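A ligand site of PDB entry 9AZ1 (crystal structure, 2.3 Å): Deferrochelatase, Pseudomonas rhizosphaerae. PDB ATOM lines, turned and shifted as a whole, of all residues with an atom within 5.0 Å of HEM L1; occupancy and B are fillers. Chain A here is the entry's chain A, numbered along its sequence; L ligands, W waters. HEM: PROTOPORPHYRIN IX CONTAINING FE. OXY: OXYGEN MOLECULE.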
ATOM      1  N   ASN A 195       6.909  38.815 -22.009  1.00  0.00           N
ATOM      2  CA  ASN A 195       5.498  38.898 -22.343  1.00  0.00           C
ATOM      3  C   ASN A 195       4.848  40.019 -21.551  1.00  0.00           C
ATOM      4  O   ASN A 195       5.519  40.785 -20.840  1.00  0.00           O
ATOM      5  CB  ASN A 195       4.815  37.546 -22.106  1.00  0.00           C
ATOM      6  CG  ASN A 195       5.143  36.969 -20.735  1.00  0.00           C
ATOM      7  OD1 ASN A 195       5.035  37.646 -19.721  1.00  0.00           O
ATOM      8  ND2 ASN A 195       5.538  35.704 -20.717  1.00  0.00           N
ATOM      9  N   LEU A 197       3.063  39.672 -19.003  1.00  0.00           N
ATOM     10  CA  LEU A 197       3.081  39.323 -17.588  1.00  0.00           C
ATOM     11  C   LEU A 197       4.434  39.589 -16.940  1.00  0.00           C
ATOM     12  O   LEU A 197       4.622  39.246 -15.771  1.00  0.00           O
ATOM     13  CB  LEU A 197       2.695  37.847 -17.406  1.00  0.00           C
ATOM     14  CG  LEU A 197       1.234  37.480 -17.687  1.00  0.00           C
ATOM     15  CD1 LEU A 197       0.881  36.150 -17.041  1.00  0.00           C
ATOM     16  CD2 LEU A 197       0.297  38.568 -17.204  1.00  0.00           C
ATOM     17  N   PHE A 199       7.410  38.280 -17.581  1.00  0.00           N
ATOM     18  CA  PHE A 199       8.327  37.159 -17.521  1.00  0.00           C
ATOM     19  C   PHE A 199       8.978  36.925 -18.880  1.00  0.00           C
ATOM     20  O   PHE A 199       8.362  37.155 -19.930  1.00  0.00           O
ATOM     21  CB  PHE A 199       7.613  35.889 -17.071  1.00  0.00           C
ATOM     22  CG  PHE A 199       7.438  35.776 -15.588  1.00  0.00           C
ATOM     23  CD1 PHE A 199       6.505  36.563 -14.930  1.00  0.00           C
ATOM     24  CD2 PHE A 199       8.192  34.878 -14.851  1.00  0.00           C
ATOM     25  CE1 PHE A 199       6.335  36.467 -13.558  1.00  0.00           C
ATOM     26  CE2 PHE A 199       8.029  34.780 -13.486  1.00  0.00           C
ATOM     27  CZ  PHE A 199       7.103  35.565 -12.836  1.00  0.00           C
ATOM     28  N   ARG A 200      10.222  36.466 -18.853  1.00  0.00           N
ATOM     29  CA  ARG A 200      10.886  36.046 -20.084  1.00  0.00           C
ATOM     30  C   ARG A 200      10.163  34.847 -20.679  1.00  0.00           C
ATOM     31  O   ARG A 200       9.860  33.881 -19.983  1.00  0.00           O
ATOM     32  CB  ARG A 200      12.358  35.702 -19.807  1.00  0.00           C
ATOM     33  CG  ARG A 200      13.177  36.879 -19.283  1.00  0.00           C
ATOM     34  CD  ARG A 200      14.630  36.480 -19.066  1.00  0.00           C
ATOM     35  NE  ARG A 200      15.326  37.417 -18.195  1.00  0.00           N
ATOM     36  CZ  ARG A 200      16.645  37.492 -18.081  1.00  0.00           C
ATOM     37  NH1 ARG A 200      17.455  36.711 -18.784  1.00  0.00           N
ATOM     38  NH2 ARG A 200      17.176  38.391 -17.255  1.00  0.00           N
ATOM     39  N   ASP A 201       9.883  34.913 -21.986  1.00  0.00           N
ATOM     40  CA  ASP A 201       9.062  33.921 -22.669  1.00  0.00           C
ATOM     41  C   ASP A 201       9.889  33.256 -23.758  1.00  0.00           C
ATOM     42  O   ASP A 201      10.337  33.925 -24.702  1.00  0.00           O
ATOM     43  CB  ASP A 201       7.807  34.563 -23.263  1.00  0.00           C
ATOM     44  CG  ASP A 201       6.668  33.572 -23.422  1.00  0.00           C
ATOM     45  OD1 ASP A 201       6.922  32.451 -23.915  1.00  0.00           O
ATOM     46  OD2 ASP A 201       5.527  33.905 -23.048  1.00  0.00           O
ATOM     47  N   GLY A 202      10.081  31.945 -23.639  1.00  0.00           N
ATOM     48  CA  GLY A 202      10.855  31.181 -24.599  1.00  0.00           C
ATOM     49  C   GLY A 202      12.192  30.661 -24.099  1.00  0.00           C
ATOM     50  O   GLY A 202      13.008  30.209 -24.921  1.00  0.00           O
ATOM     51  N   SER A 203      12.452  30.703 -22.796  1.00  0.00           N
ATOM     52  CA  SER A 203      13.766  30.319 -22.282  1.00  0.00           C
ATOM     53  C   SER A 203      14.037  28.838 -22.516  1.00  0.00           C
ATOM     54  O   SER A 203      15.088  28.463 -23.031  1.00  0.00           O
ATOM     55  CB  SER A 203      13.866  30.656 -20.799  1.00  0.00           C
ATOM     56  OG  SER A 203      13.468  31.995 -20.562  1.00  0.00           O
ATOM     57  N   ALA A 204      13.096  27.982 -22.129  1.00  0.00           N
ATOM     58  CA  ALA A 204      13.245  26.536 -22.250  1.00  0.00           C
ATOM     59  C   ALA A 204      12.804  26.007 -23.610  1.00  0.00           C
ATOM     60  O   ALA A 204      12.496  24.813 -23.731  1.00  0.00           O
ATOM     61  CB  ALA A 204      12.479  25.827 -21.132  1.00  0.00           C
ATOM     62  N   ASN A 205      12.745  26.871 -24.627  1.00  0.00           N
ATOM     63  CA  ASN A 205      12.413  26.403 -25.958  1.00  0.00           C
ATOM     64  C   ASN A 205      13.503  25.456 -26.459  1.00  0.00           C
ATOM     65  O   ASN A 205      14.684  25.663 -26.160  1.00  0.00           O
ATOM     66  CB  ASN A 205      12.266  27.586 -26.928  1.00  0.00           C
ATOM     67  CG  ASN A 205      10.846  27.751 -27.442  1.00  0.00           C
ATOM     68  OD1 ASN A 205      10.043  26.814 -27.391  1.00  0.00           O
ATOM     69  ND2 ASN A 205      10.548  28.936 -27.944  1.00  0.00           N
ATOM     70  N   ILE A 241      -4.744  34.379 -26.177  1.00  0.00           N
ATOM     71  CA  ILE A 241      -5.003  34.257 -24.742  1.00  0.00           C
ATOM     72  C   ILE A 241      -4.992  35.644 -24.129  1.00  0.00           C
ATOM     73  O   ILE A 241      -4.004  36.388 -24.252  1.00  0.00           O
ATOM     74  CB  ILE A 241      -3.966  33.355 -24.062  1.00  0.00           C
ATOM     75  CG1 ILE A 241      -3.728  32.084 -24.890  1.00  0.00           C
ATOM     76  CG2 ILE A 241      -4.410  32.995 -22.654  1.00  0.00           C
ATOM     77  CD1 ILE A 241      -2.397  31.430 -24.624  1.00  0.00           C
ATOM     78  N   ASN A 243      -4.870  38.259 -21.033  1.00  0.00           N
ATOM     79  CA  ASN A 243      -4.286  38.371 -19.698  1.00  0.00           C
ATOM     80  C   ASN A 243      -5.114  39.343 -18.867  1.00  0.00           C
ATOM     81  O   ASN A 243      -5.455  40.435 -19.329  1.00  0.00           O
ATOM     82  CB  ASN A 243      -2.841  38.858 -19.780  1.00  0.00           C
ATOM     83  CG  ASN A 243      -1.906  37.819 -20.372  1.00  0.00           C
ATOM     84  OD1 ASN A 243      -2.216  36.625 -20.398  1.00  0.00           O
ATOM     85  ND2 ASN A 243      -0.750  38.267 -20.847  1.00  0.00           N
ATOM     86  N   PHE A 260       4.642  30.231 -12.136  1.00  0.00           N
ATOM     87  CA  PHE A 260       5.393  29.912 -13.340  1.00  0.00           C
ATOM     88  C   PHE A 260       6.514  28.915 -13.097  1.00  0.00           C
ATOM     89  O   PHE A 260       6.788  28.092 -13.977  1.00  0.00           O
ATOM     90  CB  PHE A 260       5.984  31.192 -13.948  1.00  0.00           C
ATOM     91  CG  PHE A 260       5.057  31.889 -14.903  1.00  0.00           C
ATOM     92  CD1 PHE A 260       4.559  31.219 -16.005  1.00  0.00           C
ATOM     93  CD2 PHE A 260       4.683  33.199 -14.692  1.00  0.00           C
ATOM     94  CE1 PHE A 260       3.710  31.856 -16.888  1.00  0.00           C
ATOM     95  CE2 PHE A 260       3.835  33.842 -15.562  1.00  0.00           C
ATOM     96  CZ  PHE A 260       3.343  33.170 -16.671  1.00  0.00           C
ATOM     97  N   ARG A 262       9.639  30.114 -12.397  1.00  0.00           N
ATOM     98  CA  ARG A 262      10.830  30.841 -12.827  1.00  0.00           C
ATOM     99  C   ARG A 262      10.902  32.171 -12.102  1.00  0.00           C
ATOM    100  O   ARG A 262       9.876  32.785 -11.789  1.00  0.00           O
ATOM    101  CB  ARG A 262      10.833  31.077 -14.345  1.00  0.00           C
ATOM    102  CG  ARG A 262      11.009  29.823 -15.179  1.00  0.00           C
ATOM    103  CD  ARG A 262      12.472  29.590 -15.505  1.00  0.00           C
ATOM    104  NE  ARG A 262      12.653  28.506 -16.460  1.00  0.00           N
ATOM    105  CZ  ARG A 262      13.804  28.213 -17.042  1.00  0.00           C
ATOM    106  NH1 ARG A 262      14.905  28.906 -16.800  1.00  0.00           N
ATOM    107  NH2 ARG A 262      13.856  27.191 -17.896  1.00  0.00           N
ATOM    108  N   TYR A 281      13.888  18.248 -11.565  1.00  0.00           N
ATOM    109  CA  TYR A 281      12.725  17.699 -10.892  1.00  0.00           C
ATOM    110  C   TYR A 281      13.028  16.384 -10.187  1.00  0.00           C
ATOM    111  O   TYR A 281      12.274  15.983  -9.288  1.00  0.00           O
ATOM    112  CB  TYR A 281      11.577  17.503 -11.880  1.00  0.00           C
ATOM    113  CG  TYR A 281      11.067  18.789 -12.492  1.00  0.00           C
ATOM    114  CD1 TYR A 281      10.490  18.804 -13.755  1.00  0.00           C
ATOM    115  CD2 TYR A 281      11.170  19.996 -11.804  1.00  0.00           C
ATOM    116  CE1 TYR A 281      10.041  19.979 -14.323  1.00  0.00           C
ATOM    117  CE2 TYR A 281      10.714  21.173 -12.365  1.00  0.00           C
ATOM    118  CZ  TYR A 281      10.151  21.159 -13.623  1.00  0.00           C
ATOM    119  OH  TYR A 281       9.695  22.335 -14.184  1.00  0.00           O
ATOM    120  N   HIS A 295       3.702  26.319 -14.041  1.00  0.00           N
ATOM    121  CA  HIS A 295       3.465  26.328 -15.488  1.00  0.00           C
ATOM    122  C   HIS A 295       4.493  25.482 -16.224  1.00  0.00           C
ATOM    123  O   HIS A 295       4.143  24.652 -17.066  1.00  0.00           O
ATOM    124  CB  HIS A 295       3.467  27.772 -16.001  1.00  0.00           C
ATOM    125  CG  HIS A 295       3.167  27.884 -17.463  1.00  0.00           C
ATOM    126  ND1 HIS A 295       1.923  27.618 -17.998  1.00  0.00           N
ATOM    127  CD2 HIS A 295       3.954  28.250 -18.503  1.00  0.00           C
ATOM    128  CE1 HIS A 295       1.955  27.806 -19.298  1.00  0.00           C
ATOM    129  NE2 HIS A 295       3.174  28.194 -19.644  1.00  0.00           N
ATOM    130  N   ILE A 296       5.786  25.676 -15.915  1.00  0.00           N
ATOM    131  CA  ILE A 296       6.826  24.969 -16.647  1.00  0.00           C
ATOM    132  C   ILE A 296       6.880  23.505 -16.230  1.00  0.00           C
ATOM    133  O   ILE A 296       7.251  22.638 -17.037  1.00  0.00           O
ATOM    134  CB  ILE A 296       8.183  25.659 -16.446  1.00  0.00           C
ATOM    135  CG1 ILE A 296       8.645  25.570 -14.994  1.00  0.00           C
ATOM    136  CG2 ILE A 296       8.104  27.113 -16.897  1.00  0.00           C
ATOM    137  CD1 ILE A 296      10.079  26.001 -14.782  1.00  0.00           C
ATOM    138  N   ALA A 299       3.913  21.841 -18.047  1.00  0.00           N
ATOM    139  CA  ALA A 299       4.077  21.833 -19.494  1.00  0.00           C
ATOM    140  C   ALA A 299       5.218  20.922 -19.944  1.00  0.00           C
ATOM    141  O   ALA A 299       5.141  20.338 -21.026  1.00  0.00           O
ATOM    142  CB  ALA A 299       4.323  23.259 -20.000  1.00  0.00           C
ATOM    143  N   ASN A 300       6.261  20.773 -19.131  1.00  0.00           N
ATOM    144  CA  ASN A 300       7.415  19.952 -19.468  1.00  0.00           C
ATOM    145  C   ASN A 300       7.910  19.246 -18.215  1.00  0.00           C
ATOM    146  O   ASN A 300       8.764  19.771 -17.483  1.00  0.00           O
ATOM    147  CB  ASN A 300       8.523  20.785 -20.110  1.00  0.00           C
ATOM    148  CG  ASN A 300       9.666  19.927 -20.640  1.00  0.00           C
ATOM    149  OD1 ASN A 300       9.562  18.712 -20.720  1.00  0.00           O
ATOM    150  ND2 ASN A 300      10.771  20.580 -20.991  1.00  0.00           N
ATOM    151  N   ARG A 302       9.892  16.855 -18.006  1.00  0.00           N
ATOM    152  CA  ARG A 302      11.281  16.440 -18.202  1.00  0.00           C
ATOM    153  C   ARG A 302      11.473  14.967 -17.848  1.00  0.00           C
ATOM    154  O   ARG A 302      12.311  14.592 -17.028  1.00  0.00           O
ATOM    155  CB  ARG A 302      12.231  17.349 -17.422  1.00  0.00           C
ATOM    156  CG  ARG A 302      12.041  18.819 -17.758  1.00  0.00           C
ATOM    157  CD  ARG A 302      13.086  19.713 -17.108  1.00  0.00           C
ATOM    158  NE  ARG A 302      12.860  21.112 -17.433  1.00  0.00           N
ATOM    159  CZ  ARG A 302      13.331  21.710 -18.516  1.00  0.00           C
ATOM    160  NH1 ARG A 302      14.087  21.073 -19.388  1.00  0.00           N
ATOM    161  NH2 ARG A 302      13.031  22.996 -18.729  1.00  0.00           N
ATOM    162  N   ILE A 311       7.602  21.440 -27.725  1.00  0.00           N
ATOM    163  CA  ILE A 311       7.065  22.357 -28.723  1.00  0.00           C
ATOM    164  C   ILE A 311       7.979  23.562 -28.837  1.00  0.00           C
ATOM    165  O   ILE A 311       8.646  23.961 -27.871  1.00  0.00           O
ATOM    166  CB  ILE A 311       5.626  22.800 -28.373  1.00  0.00           C
ATOM    167  CG1 ILE A 311       5.582  23.461 -26.993  1.00  0.00           C
ATOM    168  CG2 ILE A 311       4.662  21.625 -28.437  1.00  0.00           C
ATOM    169  CD1 ILE A 311       4.372  24.322 -26.760  1.00  0.00           C
ATOM    170  N   ARG A 313       7.865  27.383 -29.308  1.00  0.00           N
ATOM    171  CA  ARG A 313       6.946  28.498 -29.162  1.00  0.00           C
ATOM    172  C   ARG A 313       7.505  29.752 -29.834  1.00  0.00           C
ATOM    173  O   ARG A 313       8.706  29.990 -29.841  1.00  0.00           O
ATOM    174  CB  ARG A 313       6.655  28.781 -27.692  1.00  0.00           C
ATOM    175  CG  ARG A 313       5.893  27.672 -26.995  1.00  0.00           C
ATOM    176  CD  ARG A 313       5.950  27.817 -25.489  1.00  0.00           C
ATOM    177  NE  ARG A 313       7.261  27.464 -24.958  1.00  0.00           N
ATOM    178  CZ  ARG A 313       7.930  28.197 -24.074  1.00  0.00           C
ATOM    179  NH1 ARG A 313       7.435  29.321 -23.596  1.00  0.00           N
ATOM    180  NH2 ARG A 313       9.133  27.792 -23.671  1.00  0.00           N
ATOM    181  N   LEU A 332      -1.409  37.426 -24.756  1.00  0.00           N
ATOM    182  CA  LEU A 332      -0.360  36.740 -25.498  1.00  0.00           C
ATOM    183  C   LEU A 332      -0.950  36.112 -26.750  1.00  0.00           C
ATOM    184  O   LEU A 332      -1.940  35.375 -26.685  1.00  0.00           O
ATOM    185  CB  LEU A 332       0.290  35.663 -24.632  1.00  0.00           C
ATOM    186  CG  LEU A 332       1.561  35.002 -25.192  1.00  0.00           C
ATOM    187  CD1 LEU A 332       2.764  35.922 -25.024  1.00  0.00           C
ATOM    188  CD2 LEU A 332       1.804  33.662 -24.535  1.00  0.00           C
ATOM    189  N   PHE A 334      -0.324  33.400 -28.654  1.00  0.00           N
ATOM    190  CA  PHE A 334       0.446  32.164 -28.548  1.00  0.00           C
ATOM    191  C   PHE A 334       0.527  31.479 -29.902  1.00  0.00           C
ATOM    192  O   PHE A 334      -0.493  31.190 -30.529  1.00  0.00           O
ATOM    193  CB  PHE A 334      -0.198  31.242 -27.513  1.00  0.00           C
ATOM    194  CG  PHE A 334       0.558  29.963 -27.299  1.00  0.00           C
ATOM    195  CD1 PHE A 334       1.615  29.914 -26.401  1.00  0.00           C
ATOM    196  CD2 PHE A 334       0.208  28.803 -27.977  1.00  0.00           C
ATOM    197  CE1 PHE A 334       2.309  28.734 -26.186  1.00  0.00           C
ATOM    198  CE2 PHE A 334       0.900  27.626 -27.778  1.00  0.00           C
ATOM    199  CZ  PHE A 334       1.948  27.588 -26.877  1.00  0.00           C
ATOM    200  N   PHE A 345       1.012  20.620 -28.839  1.00  0.00           N
ATOM    201  CA  PHE A 345       0.244  21.583 -28.060  1.00  0.00           C
ATOM    202  C   PHE A 345      -0.947  20.928 -27.359  1.00  0.00           C
ATOM    203  O   PHE A 345      -1.278  21.282 -26.220  1.00  0.00           O
ATOM    204  CB  PHE A 345      -0.226  22.723 -28.957  1.00  0.00           C
ATOM    205  CG  PHE A 345      -1.387  23.501 -28.395  1.00  0.00           C
ATOM    206  CD1 PHE A 345      -1.181  24.482 -27.446  1.00  0.00           C
ATOM    207  CD2 PHE A 345      -2.681  23.234 -28.810  1.00  0.00           C
ATOM    208  CE1 PHE A 345      -2.248  25.197 -26.921  1.00  0.00           C
ATOM    209  CE2 PHE A 345      -3.747  23.935 -28.293  1.00  0.00           C
ATOM    210  CZ  PHE A 345      -3.527  24.918 -27.346  1.00  0.00           C
ATOM    211  N   VAL A 348       0.216  19.100 -24.262  1.00  0.00           N
ATOM    212  CA  VAL A 348       0.757  20.024 -23.268  1.00  0.00           C
ATOM    213  C   VAL A 348      -0.352  20.851 -22.630  1.00  0.00           C
ATOM    214  O   VAL A 348      -0.381  21.034 -21.406  1.00  0.00           O
ATOM    215  CB  VAL A 348       1.833  20.922 -23.900  1.00  0.00           C
ATOM    216  CG1 VAL A 348       2.320  21.950 -22.899  1.00  0.00           C
ATOM    217  CG2 VAL A 348       3.000  20.074 -24.397  1.00  0.00           C
ATOM    218  N   GLN A 349      -1.292  21.349 -23.450  1.00  0.00           N
ATOM    219  CA  GLN A 349      -2.407  22.110 -22.898  1.00  0.00           C
ATOM    220  C   GLN A 349      -3.305  21.233 -22.023  1.00  0.00           C
ATOM    221  O   GLN A 349      -3.874  21.718 -21.039  1.00  0.00           O
ATOM    222  CB  GLN A 349      -3.221  22.744 -24.023  1.00  0.00           C
ATOM    223  CG  GLN A 349      -4.403  23.577 -23.550  1.00  0.00           C
ATOM    224  CD  GLN A 349      -4.012  24.649 -22.550  1.00  0.00           C
ATOM    225  OE1 GLN A 349      -3.312  25.594 -22.892  1.00  0.00           O
ATOM    226  NE2 GLN A 349      -4.465  24.500 -21.314  1.00  0.00           N
ATOM    227  N   LEU A 352      -1.848  21.276 -18.824  1.00  0.00           N
ATOM    228  CA  LEU A 352      -1.986  22.600 -18.221  1.00  0.00           C
ATOM    229  C   LEU A 352      -3.404  22.892 -17.745  1.00  0.00           C
ATOM    230  O   LEU A 352      -3.620  23.914 -17.097  1.00  0.00           O
ATOM    231  CB  LEU A 352      -1.561  23.679 -19.220  1.00  0.00           C
ATOM    232  CG  LEU A 352      -0.049  23.837 -19.460  1.00  0.00           C
ATOM    233  CD1 LEU A 352       0.214  24.900 -20.507  1.00  0.00           C
ATOM    234  CD2 LEU A 352       0.666  24.168 -18.158  1.00  0.00           C
ATOM    235  N   LEU A 357      -2.242  29.370 -13.164  1.00  0.00           N
ATOM    236  CA  LEU A 357      -2.117  30.502 -14.065  1.00  0.00           C
ATOM    237  C   LEU A 357      -3.438  30.858 -14.730  1.00  0.00           C
ATOM    238  O   LEU A 357      -3.598  32.000 -15.178  1.00  0.00           O
ATOM    239  CB  LEU A 357      -1.050  30.214 -15.125  1.00  0.00           C
ATOM    240  CG  LEU A 357      -0.665  31.344 -16.091  1.00  0.00           C
ATOM    241  CD1 LEU A 357      -0.138  32.540 -15.329  1.00  0.00           C
ATOM    242  CD2 LEU A 357       0.342  30.854 -17.115  1.00  0.00           C
ATOM    243  N   LEU A 361      -5.723  33.999 -17.061  1.00  0.00           N
ATOM    244  CA  LEU A 361      -5.746  33.648 -18.470  1.00  0.00           C
ATOM    245  C   LEU A 361      -7.181  33.473 -18.954  1.00  0.00           C
ATOM    246  O   LEU A 361      -8.064  33.095 -18.179  1.00  0.00           O
ATOM    247  CB  LEU A 361      -4.955  32.357 -18.731  1.00  0.00           C
ATOM    248  CG  LEU A 361      -3.498  32.467 -19.189  1.00  0.00           C
ATOM    249  CD1 LEU A 361      -2.733  33.525 -18.410  1.00  0.00           C
ATOM    250  CD2 LEU A 361      -2.814  31.112 -19.077  1.00  0.00           C
HETATM  251  CHA HEM L   1       7.229  28.012 -20.408  1.00  0.00           C
HETATM  252  CHB HEM L   1       3.898  25.856 -23.207  1.00  0.00           C
HETATM  253  CHC HEM L   1       0.818  29.509 -22.312  1.00  0.00           C
HETATM  254  CHD HEM L   1       4.414  31.971 -20.175  1.00  0.00           C
HETATM  255  C1A HEM L   1       6.608  27.093 -21.229  1.00  0.00           C
HETATM  256  C2A HEM L   1       7.153  25.838 -21.724  1.00  0.00           C
HETATM  257  C3A HEM L   1       6.232  25.257 -22.491  1.00  0.00           C
HETATM  258  C4A HEM L   1       5.063  26.106 -22.520  1.00  0.00           C
HETATM  259  CMA HEM L   1       6.381  23.912 -23.217  1.00  0.00           C
HETATM  260  CAA HEM L   1       8.547  25.256 -21.432  1.00  0.00           C
HETATM  261  CBA HEM L   1       8.652  24.862 -19.968  1.00  0.00           C
HETATM  262  CGA HEM L   1       9.893  24.027 -19.752  1.00  0.00           C
HETATM  263  O1A HEM L   1      10.371  23.410 -20.732  1.00  0.00           O
HETATM  264  O2A HEM L   1      10.401  23.989 -18.601  1.00  0.00           O
HETATM  265  C1B HEM L   1       2.752  26.629 -23.169  1.00  0.00           C
HETATM  266  C2B HEM L   1       1.473  26.274 -23.754  1.00  0.00           C
HETATM  267  C3B HEM L   1       0.617  27.272 -23.507  1.00  0.00           C
HETATM  268  C4B HEM L   1       1.324  28.295 -22.771  1.00  0.00           C
HETATM  269  CMB HEM L   1       1.147  24.970 -24.512  1.00  0.00           C
HETATM  270  CAB HEM L   1      -0.859  27.249 -23.984  1.00  0.00           C
HETATM  271  CBB HEM L   1      -1.728  28.206 -23.670  1.00  0.00           C
HETATM  272  C1C HEM L   1       1.528  30.512 -21.693  1.00  0.00           C
HETATM  273  C2C HEM L   1       1.013  31.817 -21.349  1.00  0.00           C
HETATM  274  C3C HEM L   1       1.991  32.522 -20.754  1.00  0.00           C
HETATM  275  C4C HEM L   1       3.172  31.666 -20.698  1.00  0.00           C
HETATM  276  CMC HEM L   1      -0.410  32.332 -21.623  1.00  0.00           C
HETATM  277  CAC HEM L   1       1.803  33.967 -20.255  1.00  0.00           C
HETATM  278  CBC HEM L   1       2.783  34.663 -19.656  1.00  0.00           C
HETATM  279  C1D HEM L   1       5.474  31.105 -20.007  1.00  0.00           C
HETATM  280  C2D HEM L   1       6.704  31.373 -19.292  1.00  0.00           C
HETATM  281  C3D HEM L   1       7.482  30.296 -19.357  1.00  0.00           C
HETATM  282  C4D HEM L   1       6.771  29.284 -20.113  1.00  0.00           C
HETATM  283  CMD HEM L   1       7.058  32.701 -18.570  1.00  0.00           C
HETATM  284  CAD HEM L   1       8.885  30.148 -18.724  1.00  0.00           C
HETATM  285  CBD HEM L   1       9.942  30.632 -19.699  1.00  0.00           C
HETATM  286  CGD HEM L   1      10.144  29.614 -20.788  1.00  0.00           C
HETATM  287  O1D HEM L   1      10.748  28.546 -20.505  1.00  0.00           O
HETATM  288  O2D HEM L   1       9.700  29.863 -21.933  1.00  0.00           O
HETATM  289  NA  HEM L   1       5.331  27.226 -21.742  1.00  0.00           N
HETATM  290  NB  HEM L   1       2.619  27.868 -22.581  1.00  0.00           N
HETATM  291  NC  HEM L   1       2.844  30.458 -21.274  1.00  0.00           N
HETATM  292  ND  HEM L   1       5.557  29.813 -20.489  1.00  0.00           N
HETATM  293 FE   HEM L   1       4.091  28.853 -21.522  1.00  0.00          FE
HETATM  294  O1  OXY L   2       4.587  30.448 -23.744  1.00  0.00           O
HETATM  295  O2  OXY L   2       4.504  31.136 -24.738  1.00  0.00           O
HETATM  296  O   HOH W   1      11.118  26.667 -18.245  1.00  0.00           O
HETATM  297  O   HOH W   2      10.094  22.065 -17.006  1.00  0.00           O
HETATM  298  O   HOH W   3      -4.658  27.672 -24.233  1.00  0.00           O
HETATM  299  O   HOH W   4       6.633  20.591 -23.627  1.00  0.00           O
HETATM  300  O   HOH W   5      10.360  33.106 -17.317  1.00  0.00           O
HETATM  301  O   HOH W   6      10.849  22.687 -23.450  1.00  0.00           O
HETATM  302  O   HOH W   7       8.836  25.040 -25.430  1.00  0.00           O
HETATM  303  O   HOH W   8      -3.994  29.193 -21.718  1.00  0.00           O
HETATM  304  O   HOH W   9       1.490  37.253 -21.450  1.00  0.00           O
HETATM  305  O   HOH W  10       8.750  22.262 -24.948  1.00  0.00           O
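ND2 of Asn 195 touches CBC of HEM L1, 3.1 Å away. Leu 197 touches HEM L1. Phe 199 touches HEM L1 (CB to CMD, 3.6 Å). O of Arg 200 touches CBD of HEM L1, 3.3 Å away. OD2 of Asp 201 touches CHD of HEM L1, at 3.6 Å. Ile 241 touches HEM L1 (CD1 to CBB, 3.4 Å). Phe 260 touches HEM L1 (CE1 to CHD, 3.4 Å). Ile 296 touches HEM L1. Ala 299 touches HEM L1 (CB to C3A, 3.7 Å). CG1 of Ile 311 touches CMA of HEM L1, at 3.9 Å. Leu 332 touches HEM L1. CZ of Phe 334 touches C2B of HEM L1, at 3.4 Å. Phe 345 touches HEM L1 (CD1 to CMB, 3.8 Å). Val 348 touches HEM L1 (CG1 to CMB, 3.6 Å). OE1 of Gln 349 touches CBB of HEM L1, 3.2 Å away. Leu 352 touches HEM L1 (CD1 to C2B, 3.7 Å). Leu 361 touches HEM L1 (CD2 to CMC, 3.7 Å). Hydrophobic or aromatic side chains within 4 Å of HEM L1: Leu 197, Phe 199, Ala 204, Ile 241, Phe 260, His 295, Ile 296, Ala 299, Ile 311, Leu 332, Phe 334, Phe 345, Val 348, Leu 352 and Leu 361. Within 4 Å of HEM L1: Asn 195, Leu 197, Phe 199, Arg 200, Asp 201, Gly 202, Ser 203, Ala 204, Ile 241, Phe 260, His 295, Ile 296, Ala 299, Asn 300, Arg 302, Ile 311, Arg 313, Leu 332, Phe 334, Phe 345, Val 348, Gln 349, Leu 352 and Leu 361.
NH1 of Arg 313 lies within salt-bridge range of OD1 of Asp 201 (3.2 Å). The backbone carbonyl oxygen (O) of Ile 311 lies close to the side-chain amide oxygen (OD1) of Asn 205 (3.2 Å). The side-chain amide oxygen of Asn 195 sits at hydrogen-bond distance from the backbone NH of Leu 197, at 2.9 Å. The backbone carbonyl oxygen of Ile 241 lies within hydrogen-bond range of the backbone NH of Leu 332 (2.8 Å). The backbone NH (N) of Arg 302 lies close to the side-chain amide oxygen (OD1) of Asn 300 (3.3 Å). O of Arg 313 lies within hydrogen-bond range of ND2 of Asn 205, at 2.8 Å. O of Phe 260 sits at hydrogen-bond distance from N of Ile 296 (3.3 Å). The side-chain amide nitrogen (ND2) of Asn 195 lies within hydrogen-bond range of the side-chain carboxylate (OD2) of Asp 201 (2.9 Å).
Water W2 lies within hydrogen-bond range of an oxygen (O2A) of HEM L1 (2.5 Å), the backbone carbonyl oxygen of Asn 300 (2.7 Å), the side-chain hydroxyl of Tyr 281 (2.9 Å), the backbone carbonyl oxygen of Ile 296 (2.9 Å) and the guanidinium group of Arg 302 (3.0 Å). Water W1 lies within hydrogen-bond range of O2A of HEM L1 (2.8 Å) and NH2 of Arg 262 (2.8 Å). Water W6 lies within hydrogen-bond range of O of Ala 204 (2.7 Å), O1A of HEM L1 (2.9 Å) and ND2 of Asn 300 (3.2 Å). Water W7 lies within hydrogen-bond range of O of Ile 311 (2.7 Å), OD1 of Asn 205 (2.9 Å) and NE of Arg 313 (2.9 Å).
NE2 of His 295 is bound to FE of HEM L1 (2.2 Å). The side-chain amide nitrogen of Asn 300 sits at hydrogen-bond distance from an oxygen (O1A) of HEM L1 (2.9 Å). O1D of HEM L1 lies within hydrogen-bond range of N of Ala 204 (2.9 Å). The guanidinium group (NH1) of Arg 313 is in hydrogen-bond range of an oxygen (O1) of OXY L2 (3.1 Å). The guanidinium group (NH2) of Arg 302 is in salt-bridge range of an oxygen (O2A) of HEM L1, 2.8 Å away. NH2 of Arg 313 lies within salt-bridge range of O2D of HEM L1, 2.8 Å away. N of Gly 202 sits at hydrogen-bond distance from O2D of HEM L1 (2.7 Å). The backbone NH (N) of Ser 203 sits at hydrogen-bond distance from an oxygen (O2D) of HEM L1 (3.0 Å).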
